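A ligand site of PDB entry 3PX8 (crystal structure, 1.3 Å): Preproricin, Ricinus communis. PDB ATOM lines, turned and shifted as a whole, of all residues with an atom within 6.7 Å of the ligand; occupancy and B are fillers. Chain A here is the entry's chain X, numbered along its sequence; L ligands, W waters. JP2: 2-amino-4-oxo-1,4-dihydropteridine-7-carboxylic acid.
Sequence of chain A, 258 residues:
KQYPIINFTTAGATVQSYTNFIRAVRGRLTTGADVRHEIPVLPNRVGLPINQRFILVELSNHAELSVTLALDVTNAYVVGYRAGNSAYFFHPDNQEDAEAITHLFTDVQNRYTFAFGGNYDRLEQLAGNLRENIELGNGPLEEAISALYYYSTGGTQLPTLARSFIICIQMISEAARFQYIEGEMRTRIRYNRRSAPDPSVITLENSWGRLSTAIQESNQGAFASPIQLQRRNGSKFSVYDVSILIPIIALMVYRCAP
Water W3 lies within hydrogen-bond range of O2 of the ligand (2.7 Å), N of Asp 121 (2.9 Å) and N of Tyr 120 (3.4 Å). Water W1 lies within hydrogen-bond range of an oxygen (O3) of the ligand and the side-chain amide oxygen of Asn 206.
Residues that only touch the ligand: Tyr 77, Ile 169, Ser 173, Asn 119, Ala 76, Phe 90 and Glu 174. Hydrophobic or aromatic side chains within 4 Å of the ligand: Tyr 77, Val 78, Phe 90, Tyr 120 and Ile 169. 11 residues have an atom within 4 Å of the ligand: Ala 76, Tyr 77, Val 78, Phe 90, Gly 118, Asn 119, Tyr 120, Ile 169, Ser 173, Glu 174 and Arg 177.
NH1 of Arg 177 is in salt-bridge range of OE1 of Glu 174, 3.1 Å away. The backbone carbonyl oxygen (O) of Asn 75 lies within hydrogen-bond range of the guanidinium group (NH2) of Arg 177, 2.8 Å away. The side-chain carboxylate (OE2) of Glu 174 lies within hydrogen-bond range of the side-chain hydroxyl (OH) of Tyr 120, 2.6 Å away. The side-chain amide oxygen (OD1) of Asn 75 sits at hydrogen-bond distance from the backbone NH (N) of Tyr 77 (2.9 Å). O of Ile 169 sits at hydrogen-bond distance from N of Glu 174. The side-chain hydroxyl (OG) of Ser 173 sits at hydrogen-bond distance from the backbone carbonyl oxygen (O) of Ala 76, at 2.8 Å. The backbone carbonyl oxygen (O) of Val 79 lies within hydrogen-bond range of the backbone NH (N) of Phe 90 (3.0 Å).
The backbone carbonyl oxygen (O) of Gly 118 is in hydrogen-bond range of a nitrogen (N1) of the ligand. The guanidinium group of Arg 177 sits at hydrogen-bond distance from an oxygen (O1) of the ligand (2.8 Å). O2 of the ligand sits at hydrogen-bond distance from N of Tyr 120, 2.8 Å away. The backbone NH (N) of Val 78 is in hydrogen-bond range of a nitrogen (N2) of the ligand (3.1 Å). A nitrogen (N1) of the ligand sits at hydrogen-bond distance from the backbone carbonyl oxygen (O) of Val 78, at 2.9 Å.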
ATOM      1  N   LEU A  71     -23.638   9.558 -12.790  1.00  0.00           N
ATOM      2  CA  LEU A  71     -22.381   8.867 -13.210  1.00  0.00           C
ATOM      3  C   LEU A  71     -21.366   8.882 -12.138  1.00  0.00           C
ATOM      4  O   LEU A  71     -21.202   9.975 -11.461  1.00  0.00           O
ATOM      5  CB  LEU A  71     -21.794   9.544 -14.462  1.00  0.00           C
ATOM      6  CG  LEU A  71     -22.444   9.159 -15.794  1.00  0.00           C
ATOM      7  CD1 LEU A  71     -23.902   9.560 -15.914  1.00  0.00           C
ATOM      8  CD2 LEU A  71     -21.606   9.803 -16.885  1.00  0.00           C
ATOM      9  N   ASN A  75     -15.076   6.130 -12.933  1.00  0.00           N
ATOM     10  CA  ASN A  75     -15.081   5.229 -14.115  1.00  0.00           C
ATOM     11  C   ASN A  75     -16.086   5.691 -15.147  1.00  0.00           C
ATOM     12  O   ASN A  75     -16.191   5.010 -16.212  1.00  0.00           O
ATOM     13  CB  ASN A  75     -15.341   3.782 -13.715  1.00  0.00           C
ATOM     14  CG  ASN A  75     -16.585   3.619 -12.882  1.00  0.00           C
ATOM     15  OD1 ASN A  75     -17.430   4.497 -12.876  1.00  0.00           O
ATOM     16  ND2 ASN A  75     -16.741   2.455 -12.259  1.00  0.00           N
ATOM     17  N   ALA A  76     -16.730   6.812 -14.987  1.00  0.00           N
ATOM     18  CA  ALA A  76     -17.821   7.341 -15.844  1.00  0.00           C
ATOM     19  C   ALA A  76     -19.046   6.408 -15.906  1.00  0.00           C
ATOM     20  O   ALA A  76     -19.866   6.596 -16.819  1.00  0.00           O
ATOM     21  CB  ALA A  76     -17.347   7.731 -17.290  1.00  0.00           C
ATOM     22  N   TYR A  77     -19.163   5.372 -15.056  1.00  0.00           N
ATOM     23  CA  TYR A  77     -20.298   4.459 -15.156  1.00  0.00           C
ATOM     24  C   TYR A  77     -21.582   5.106 -14.783  1.00  0.00           C
ATOM     25  O   TYR A  77     -21.683   5.859 -13.800  1.00  0.00           O
ATOM     26  CB  TYR A  77     -20.120   3.224 -14.289  1.00  0.00           C
ATOM     27  CG  TYR A  77     -19.448   2.089 -14.895  1.00  0.00           C
ATOM     28  CD1 TYR A  77     -18.233   2.266 -15.526  1.00  0.00           C
ATOM     29  CD2 TYR A  77     -19.951   0.783 -14.803  1.00  0.00           C
ATOM     30  CE1 TYR A  77     -17.501   1.160 -16.067  1.00  0.00           C
ATOM     31  CE2 TYR A  77     -19.253  -0.307 -15.362  1.00  0.00           C
ATOM     32  CZ  TYR A  77     -18.034  -0.095 -15.981  1.00  0.00           C
ATOM     33  OH  TYR A  77     -17.338  -1.163 -16.533  1.00  0.00           O
ATOM     34  N   VAL A  78     -22.662   4.751 -15.500  1.00  0.00           N
ATOM     35  CA  VAL A  78     -23.998   5.122 -15.049  1.00  0.00           C
ATOM     36  C   VAL A  78     -24.398   4.189 -13.909  1.00  0.00           C
ATOM     37  O   VAL A  78     -24.579   2.967 -14.104  1.00  0.00           O
ATOM     38  CB  VAL A  78     -24.971   4.960 -16.204  1.00  0.00           C
ATOM     39  CG1 VAL A  78     -26.395   5.327 -15.740  1.00  0.00           C
ATOM     40  CG2 VAL A  78     -24.553   5.898 -17.383  1.00  0.00           C
ATOM     41  N   VAL A  79     -24.647   4.754 -12.716  1.00  0.00           N
ATOM     42  CA  VAL A  79     -25.009   3.963 -11.539  1.00  0.00           C
ATOM     43  C   VAL A  79     -26.494   3.878 -11.272  1.00  0.00           C
ATOM     44  O   VAL A  79     -26.960   2.994 -10.490  1.00  0.00           O
ATOM     45  CB  VAL A  79     -24.249   4.356 -10.283  1.00  0.00           C
ATOM     46  CG1 VAL A  79     -22.707   4.314 -10.504  1.00  0.00           C
ATOM     47  CG2 VAL A  79     -24.606   5.725  -9.827  1.00  0.00           C
ATOM     48  N   GLY A  80     -27.252   4.760 -11.882  1.00  0.00           N
ATOM     49  CA  GLY A  80     -28.697   4.776 -11.585  1.00  0.00           C
ATOM     50  C   GLY A  80     -29.310   5.995 -12.199  1.00  0.00           C
ATOM     51  O   GLY A  80     -28.590   6.790 -12.917  1.00  0.00           O
ATOM     52  N   PHE A  90     -28.574   0.438 -10.180  1.00  0.00           N
ATOM     53  CA  PHE A  90     -28.094  -0.910 -10.450  1.00  0.00           C
ATOM     54  C   PHE A  90     -27.614  -1.509  -9.190  1.00  0.00           C
ATOM     55  O   PHE A  90     -27.143  -0.861  -8.225  1.00  0.00           O
ATOM     56  CB  PHE A  90     -26.984  -0.922 -11.530  1.00  0.00           C
ATOM     57  CG  PHE A  90     -27.440  -0.433 -12.815  1.00  0.00           C
ATOM     58  CD1 PHE A  90     -28.425  -1.090 -13.536  1.00  0.00           C
ATOM     59  CD2 PHE A  90     -26.845   0.729 -13.355  1.00  0.00           C
ATOM     60  CE1 PHE A  90     -28.896  -0.655 -14.743  1.00  0.00           C
ATOM     61  CE2 PHE A  90     -27.259   1.153 -14.607  1.00  0.00           C
ATOM     62  CZ  PHE A  90     -28.291   0.518 -15.302  1.00  0.00           C
ATOM     63  N   GLY A 117     -27.200  -6.078 -11.767  1.00  0.00           N
ATOM     64  CA  GLY A 117     -26.125  -5.092 -12.029  1.00  0.00           C
ATOM     65  C   GLY A 117     -26.271  -4.430 -13.406  1.00  0.00           C
ATOM     66  O   GLY A 117     -27.050  -4.809 -14.227  1.00  0.00           O
ATOM     67  N   GLY A 118     -25.409  -3.436 -13.636  1.00  0.00           N
ATOM     68  CA  GLY A 118     -25.492  -2.565 -14.830  1.00  0.00           C
ATOM     69  C   GLY A 118     -24.444  -2.776 -15.894  1.00  0.00           C
ATOM     70  O   GLY A 118     -24.308  -1.871 -16.728  1.00  0.00           O
ATOM     71  N   ASN A 119     -23.657  -3.838 -15.818  1.00  0.00           N
ATOM     72  CA  ASN A 119     -22.610  -4.053 -16.829  1.00  0.00           C
ATOM     73  C   ASN A 119     -23.256  -4.391 -18.157  1.00  0.00           C
ATOM     74  O   ASN A 119     -24.407  -4.960 -18.183  1.00  0.00           O
ATOM     75  CB  ASN A 119     -21.601  -5.133 -16.390  1.00  0.00           C
ATOM     76  CG  ASN A 119     -20.778  -4.707 -15.238  1.00  0.00           C
ATOM     77  OD1 ASN A 119     -20.632  -3.524 -14.980  1.00  0.00           O
ATOM     78  ND2 ASN A 119     -20.284  -5.677 -14.493  1.00  0.00           N
ATOM     79  N   TYR A 120     -22.555  -4.264 -19.280  1.00  0.00           N
ATOM     80  CA  TYR A 120     -23.136  -4.620 -20.558  1.00  0.00           C
ATOM     81  C   TYR A 120     -23.625  -6.042 -20.616  1.00  0.00           C
ATOM     82  O   TYR A 120     -24.676  -6.309 -21.229  1.00  0.00           O
ATOM     83  CB  TYR A 120     -22.224  -4.359 -21.759  1.00  0.00           C
ATOM     84  CG  TYR A 120     -21.915  -2.916 -22.057  1.00  0.00           C
ATOM     85  CD1 TYR A 120     -22.891  -1.918 -22.183  1.00  0.00           C
ATOM     86  CD2 TYR A 120     -20.610  -2.579 -22.323  1.00  0.00           C
ATOM     87  CE1 TYR A 120     -22.539  -0.614 -22.519  1.00  0.00           C
ATOM     88  CE2 TYR A 120     -20.294  -1.262 -22.714  1.00  0.00           C
ATOM     89  CZ  TYR A 120     -21.286  -0.290 -22.770  1.00  0.00           C
ATOM     90  OH  TYR A 120     -20.969   1.009 -23.161  1.00  0.00           O
ATOM     91  N   ASP A 121     -22.809  -6.986 -20.140  1.00  0.00           N
ATOM     92  CA  ASP A 121     -23.242  -8.387 -20.307  1.00  0.00           C
ATOM     93  C   ASP A 121     -24.633  -8.666 -19.705  1.00  0.00           C
ATOM     94  O   ASP A 121     -25.516  -9.206 -20.383  1.00  0.00           O
ATOM     95  CB  ASP A 121     -22.119  -9.394 -19.789  1.00  0.00           C
ATOM     96  CG  ASP A 121     -21.689  -9.183 -18.350  1.00  0.00           C
ATOM     97  OD1 ASP A 121     -22.216  -8.323 -17.592  1.00  0.00           O
ATOM     98  OD2 ASP A 121     -20.772  -9.931 -17.905  1.00  0.00           O
ATOM     99  N   LEU A 123     -26.938  -6.323 -18.959  1.00  0.00           N
ATOM    100  CA  LEU A 123     -27.947  -5.562 -19.673  1.00  0.00           C
ATOM    101  C   LEU A 123     -28.368  -6.114 -20.986  1.00  0.00           C
ATOM    102  O   LEU A 123     -29.525  -6.075 -21.371  1.00  0.00           O
ATOM    103  CB  LEU A 123     -27.529  -4.054 -19.798  1.00  0.00           C
ATOM    104  CG  LEU A 123     -27.427  -3.287 -18.493  1.00  0.00           C
ATOM    105  CD1 LEU A 123     -26.919  -1.933 -18.789  1.00  0.00           C
ATOM    106  CD2 LEU A 123     -28.721  -3.236 -17.747  1.00  0.00           C
ATOM    107  N   ARG A 131     -25.125  -5.306 -27.936  1.00  0.00           N
ATOM    108  CA  ARG A 131     -24.841  -3.937 -28.425  1.00  0.00           C
ATOM    109  C   ARG A 131     -24.820  -3.840 -29.944  1.00  0.00           C
ATOM    110  O   ARG A 131     -25.293  -2.879 -30.537  1.00  0.00           O
ATOM    111  CB  ARG A 131     -23.510  -3.408 -27.836  1.00  0.00           C
ATOM    112  CG  ARG A 131     -23.602  -2.982 -26.430  1.00  0.00           C
ATOM    113  CD  ARG A 131     -22.212  -2.714 -25.793  1.00  0.00           C
ATOM    114  NE  ARG A 131     -21.610  -4.050 -25.563  1.00  0.00           N
ATOM    115  CZ  ARG A 131     -20.336  -4.227 -25.292  1.00  0.00           C
ATOM    116  NH1 ARG A 131     -19.439  -3.238 -25.514  1.00  0.00           N
ATOM    117  NH2 ARG A 131     -19.854  -5.396 -24.934  1.00  0.00           N
ATOM    118  N   PHE A 165     -30.977   1.797 -21.265  1.00  0.00           N
ATOM    119  CA  PHE A 165     -29.759   2.023 -20.601  1.00  0.00           C
ATOM    120  C   PHE A 165     -28.546   1.781 -21.509  1.00  0.00           C
ATOM    121  O   PHE A 165     -27.577   2.577 -21.502  1.00  0.00           O
ATOM    122  CB  PHE A 165     -29.590   1.057 -19.420  1.00  0.00           C
ATOM    123  CG  PHE A 165     -30.471   1.328 -18.244  1.00  0.00           C
ATOM    124  CD1 PHE A 165     -30.658   2.615 -17.744  1.00  0.00           C
ATOM    125  CD2 PHE A 165     -31.096   0.280 -17.594  1.00  0.00           C
ATOM    126  CE1 PHE A 165     -31.468   2.829 -16.638  1.00  0.00           C
ATOM    127  CE2 PHE A 165     -31.912   0.493 -16.501  1.00  0.00           C
ATOM    128  CZ  PHE A 165     -32.095   1.768 -16.017  1.00  0.00           C
ATOM    129  N   ILE A 169     -25.711   4.673 -21.997  1.00  0.00           N
ATOM    130  CA  ILE A 169     -24.370   4.466 -21.575  1.00  0.00           C
ATOM    131  C   ILE A 169     -23.400   4.726 -22.739  1.00  0.00           C
ATOM    132  O   ILE A 169     -22.353   5.411 -22.581  1.00  0.00           O
ATOM    133  CB  ILE A 169     -24.167   3.011 -21.108  1.00  0.00           C
ATOM    134  CG1 ILE A 169     -24.918   2.811 -19.746  1.00  0.00           C
ATOM    135  CG2 ILE A 169     -22.673   2.738 -20.889  1.00  0.00           C
ATOM    136  CD1 ILE A 169     -25.257   1.268 -19.452  1.00  0.00           C
ATOM    137  N   GLN A 170     -23.756   4.258 -23.939  1.00  0.00           N
ATOM    138  CA  GLN A 170     -22.819   4.405 -25.021  1.00  0.00           C
ATOM    139  C   GLN A 170     -22.795   5.846 -25.525  1.00  0.00           C
ATOM    140  O   GLN A 170     -21.747   6.409 -25.885  1.00  0.00           O
ATOM    141  CB  GLN A 170     -23.119   3.490 -26.182  1.00  0.00           C
ATOM    142  CG  GLN A 170     -22.904   1.997 -25.787  1.00  0.00           C
ATOM    143  CD  GLN A 170     -23.282   1.155 -26.929  1.00  0.00           C
ATOM    144  OE1 GLN A 170     -22.454   0.831 -27.806  1.00  0.00           O
ATOM    145  NE2 GLN A 170     -24.542   0.748 -26.960  1.00  0.00           N
ATOM    146  N   SER A 173     -21.458   7.988 -21.541  1.00  0.00           N
ATOM    147  CA  SER A 173     -20.228   7.537 -20.898  1.00  0.00           C
ATOM    148  C   SER A 173     -19.193   7.106 -21.935  1.00  0.00           C
ATOM    149  O   SER A 173     -17.990   7.531 -21.814  1.00  0.00           O
ATOM    150  CB  SER A 173     -20.521   6.326 -19.996  1.00  0.00           C
ATOM    151  OG  SER A 173     -21.521   6.666 -19.075  1.00  0.00           O
ATOM    152  N   GLU A 174     -19.545   6.312 -22.931  1.00  0.00           N
ATOM    153  CA  GLU A 174     -18.540   5.872 -23.901  1.00  0.00           C
ATOM    154  C   GLU A 174     -18.067   7.031 -24.743  1.00  0.00           C
ATOM    155  O   GLU A 174     -16.868   7.131 -25.125  1.00  0.00           O
ATOM    156  CB  GLU A 174     -19.045   4.739 -24.790  1.00  0.00           C
ATOM    157  CG  GLU A 174     -19.374   3.432 -24.050  1.00  0.00           C
ATOM    158  CD  GLU A 174     -18.193   2.687 -23.444  1.00  0.00           C
ATOM    159  OE1 GLU A 174     -17.072   3.224 -23.451  1.00  0.00           O
ATOM    160  OE2 GLU A 174     -18.472   1.549 -22.980  1.00  0.00           O
ATOM    161  N   ARG A 177     -15.548   8.844 -22.732  1.00  0.00           N
ATOM    162  CA  ARG A 177     -14.289   8.123 -22.694  1.00  0.00           C
ATOM    163  C   ARG A 177     -13.504   8.171 -23.983  1.00  0.00           C
ATOM    164  O   ARG A 177     -12.268   8.144 -23.913  1.00  0.00           O
ATOM    165  CB  ARG A 177     -14.528   6.638 -22.375  1.00  0.00           C
ATOM    166  CG  ARG A 177     -15.052   6.343 -20.961  1.00  0.00           C
ATOM    167  CD  ARG A 177     -15.468   4.879 -20.870  1.00  0.00           C
ATOM    168  NE  ARG A 177     -16.086   4.649 -19.575  1.00  0.00           N
ATOM    169  CZ  ARG A 177     -17.221   3.951 -19.407  1.00  0.00           C
ATOM    170  NH1 ARG A 177     -17.901   3.421 -20.465  1.00  0.00           N
ATOM    171  NH2 ARG A 177     -17.741   3.820 -18.197  1.00  0.00           N
ATOM    172  N   GLU A 205     -14.943  -0.045 -26.698  1.00  0.00           N
ATOM    173  CA  GLU A 205     -15.679  -0.009 -25.389  1.00  0.00           C
ATOM    174  C   GLU A 205     -15.175  -1.147 -24.537  1.00  0.00           C
ATOM    175  O   GLU A 205     -14.855  -1.012 -23.354  1.00  0.00           O
ATOM    176  CB  GLU A 205     -17.183  -0.318 -25.657  1.00  0.00           C
ATOM    177  CG  GLU A 205     -17.889   0.856 -26.406  1.00  0.00           C
ATOM    178  CD  GLU A 205     -19.281   0.549 -26.757  1.00  0.00           C
ATOM    179  OE1 GLU A 205     -19.777  -0.577 -26.535  1.00  0.00           O
ATOM    180  OE2 GLU A 205     -19.965   1.469 -27.254  1.00  0.00           O
ATOM    181  N   ASN A 206     -14.995  -2.347 -25.132  1.00  0.00           N
ATOM    182  CA  ASN A 206     -14.599  -3.546 -24.355  1.00  0.00           C
ATOM    183  C   ASN A 206     -13.171  -3.428 -23.876  1.00  0.00           C
ATOM    184  O   ASN A 206     -12.801  -4.074 -22.882  1.00  0.00           O
ATOM    185  CB  ASN A 206     -14.724  -4.824 -25.189  1.00  0.00           C
ATOM    186  CG  ASN A 206     -16.138  -5.220 -25.448  1.00  0.00           C
ATOM    187  OD1 ASN A 206     -17.050  -4.810 -24.719  1.00  0.00           O
ATOM    188  ND2 ASN A 206     -16.352  -6.016 -26.507  1.00  0.00           N
ATOM    189  N   TRP A 208     -11.507  -0.560 -22.884  1.00  0.00           N
ATOM    190  CA  TRP A 208     -11.143   0.656 -22.150  1.00  0.00           C
ATOM    191  C   TRP A 208     -10.265   0.415 -20.967  1.00  0.00           C
ATOM    192  O   TRP A 208      -9.236   1.118 -20.787  1.00  0.00           O
ATOM    193  CB  TRP A 208     -12.416   1.413 -21.796  1.00  0.00           C
ATOM    194  CG  TRP A 208     -12.165   2.754 -21.116  1.00  0.00           C
ATOM    195  CD1 TRP A 208     -11.480   3.829 -21.648  1.00  0.00           C
ATOM    196  CD2 TRP A 208     -12.551   3.139 -19.796  1.00  0.00           C
ATOM    197  NE1 TRP A 208     -11.509   4.826 -20.726  1.00  0.00           N
ATOM    198  CE2 TRP A 208     -12.152   4.458 -19.610  1.00  0.00           C
ATOM    199  CE3 TRP A 208     -13.280   2.508 -18.773  1.00  0.00           C
ATOM    200  CZ2 TRP A 208     -12.446   5.165 -18.409  1.00  0.00           C
ATOM    201  CZ3 TRP A 208     -13.594   3.234 -17.641  1.00  0.00           C
ATOM    202  CH2 TRP A 208     -13.203   4.539 -17.497  1.00  0.00           C
HETATM  203  C1  JP2 L   1     -22.837   1.095 -17.001  1.00  0.00           C
HETATM  204  N1  JP2 L   1     -23.938   1.076 -16.228  1.00  0.00           N
HETATM  205  O1  JP2 L   1     -20.462   3.294 -18.212  1.00  0.00           O
HETATM  206  C2  JP2 L   1     -21.123   2.219 -17.957  1.00  0.00           C
HETATM  207  N2  JP2 L   1     -22.203   2.264 -17.205  1.00  0.00           N
HETATM  208  O2  JP2 L   1     -19.754  -3.777 -19.310  1.00  0.00           O
HETATM  209  C3  JP2 L   1     -20.549   1.007 -18.496  1.00  0.00           C
HETATM  210  N3  JP2 L   1     -22.414  -0.093 -17.496  1.00  0.00           N
HETATM  211  O3  JP2 L   1     -17.964  -2.842 -20.170  1.00  0.00           O
HETATM  212  C4  JP2 L   1     -21.267  -0.209 -18.232  1.00  0.00           C
HETATM  213  N4  JP2 L   1     -20.825  -1.430 -18.594  1.00  0.00           N
HETATM  214  C5  JP2 L   1     -19.610  -1.463 -19.242  1.00  0.00           C
HETATM  215  N5  JP2 L   1     -19.411   0.963 -19.302  1.00  0.00           N
HETATM  216  C6  JP2 L   1     -18.922  -0.238 -19.647  1.00  0.00           C
HETATM  217  C7  JP2 L   1     -19.075  -2.745 -19.630  1.00  0.00           C
HETATM  218  O   HOH W   1     -17.492  -4.977 -21.903  1.00  0.00           O
HETATM  219  O   HOH W   2     -15.483   0.039 -19.293  1.00  0.00           O
HETATM  220  O   HOH W   3     -20.012  -6.484 -19.375  1.00  0.00           O
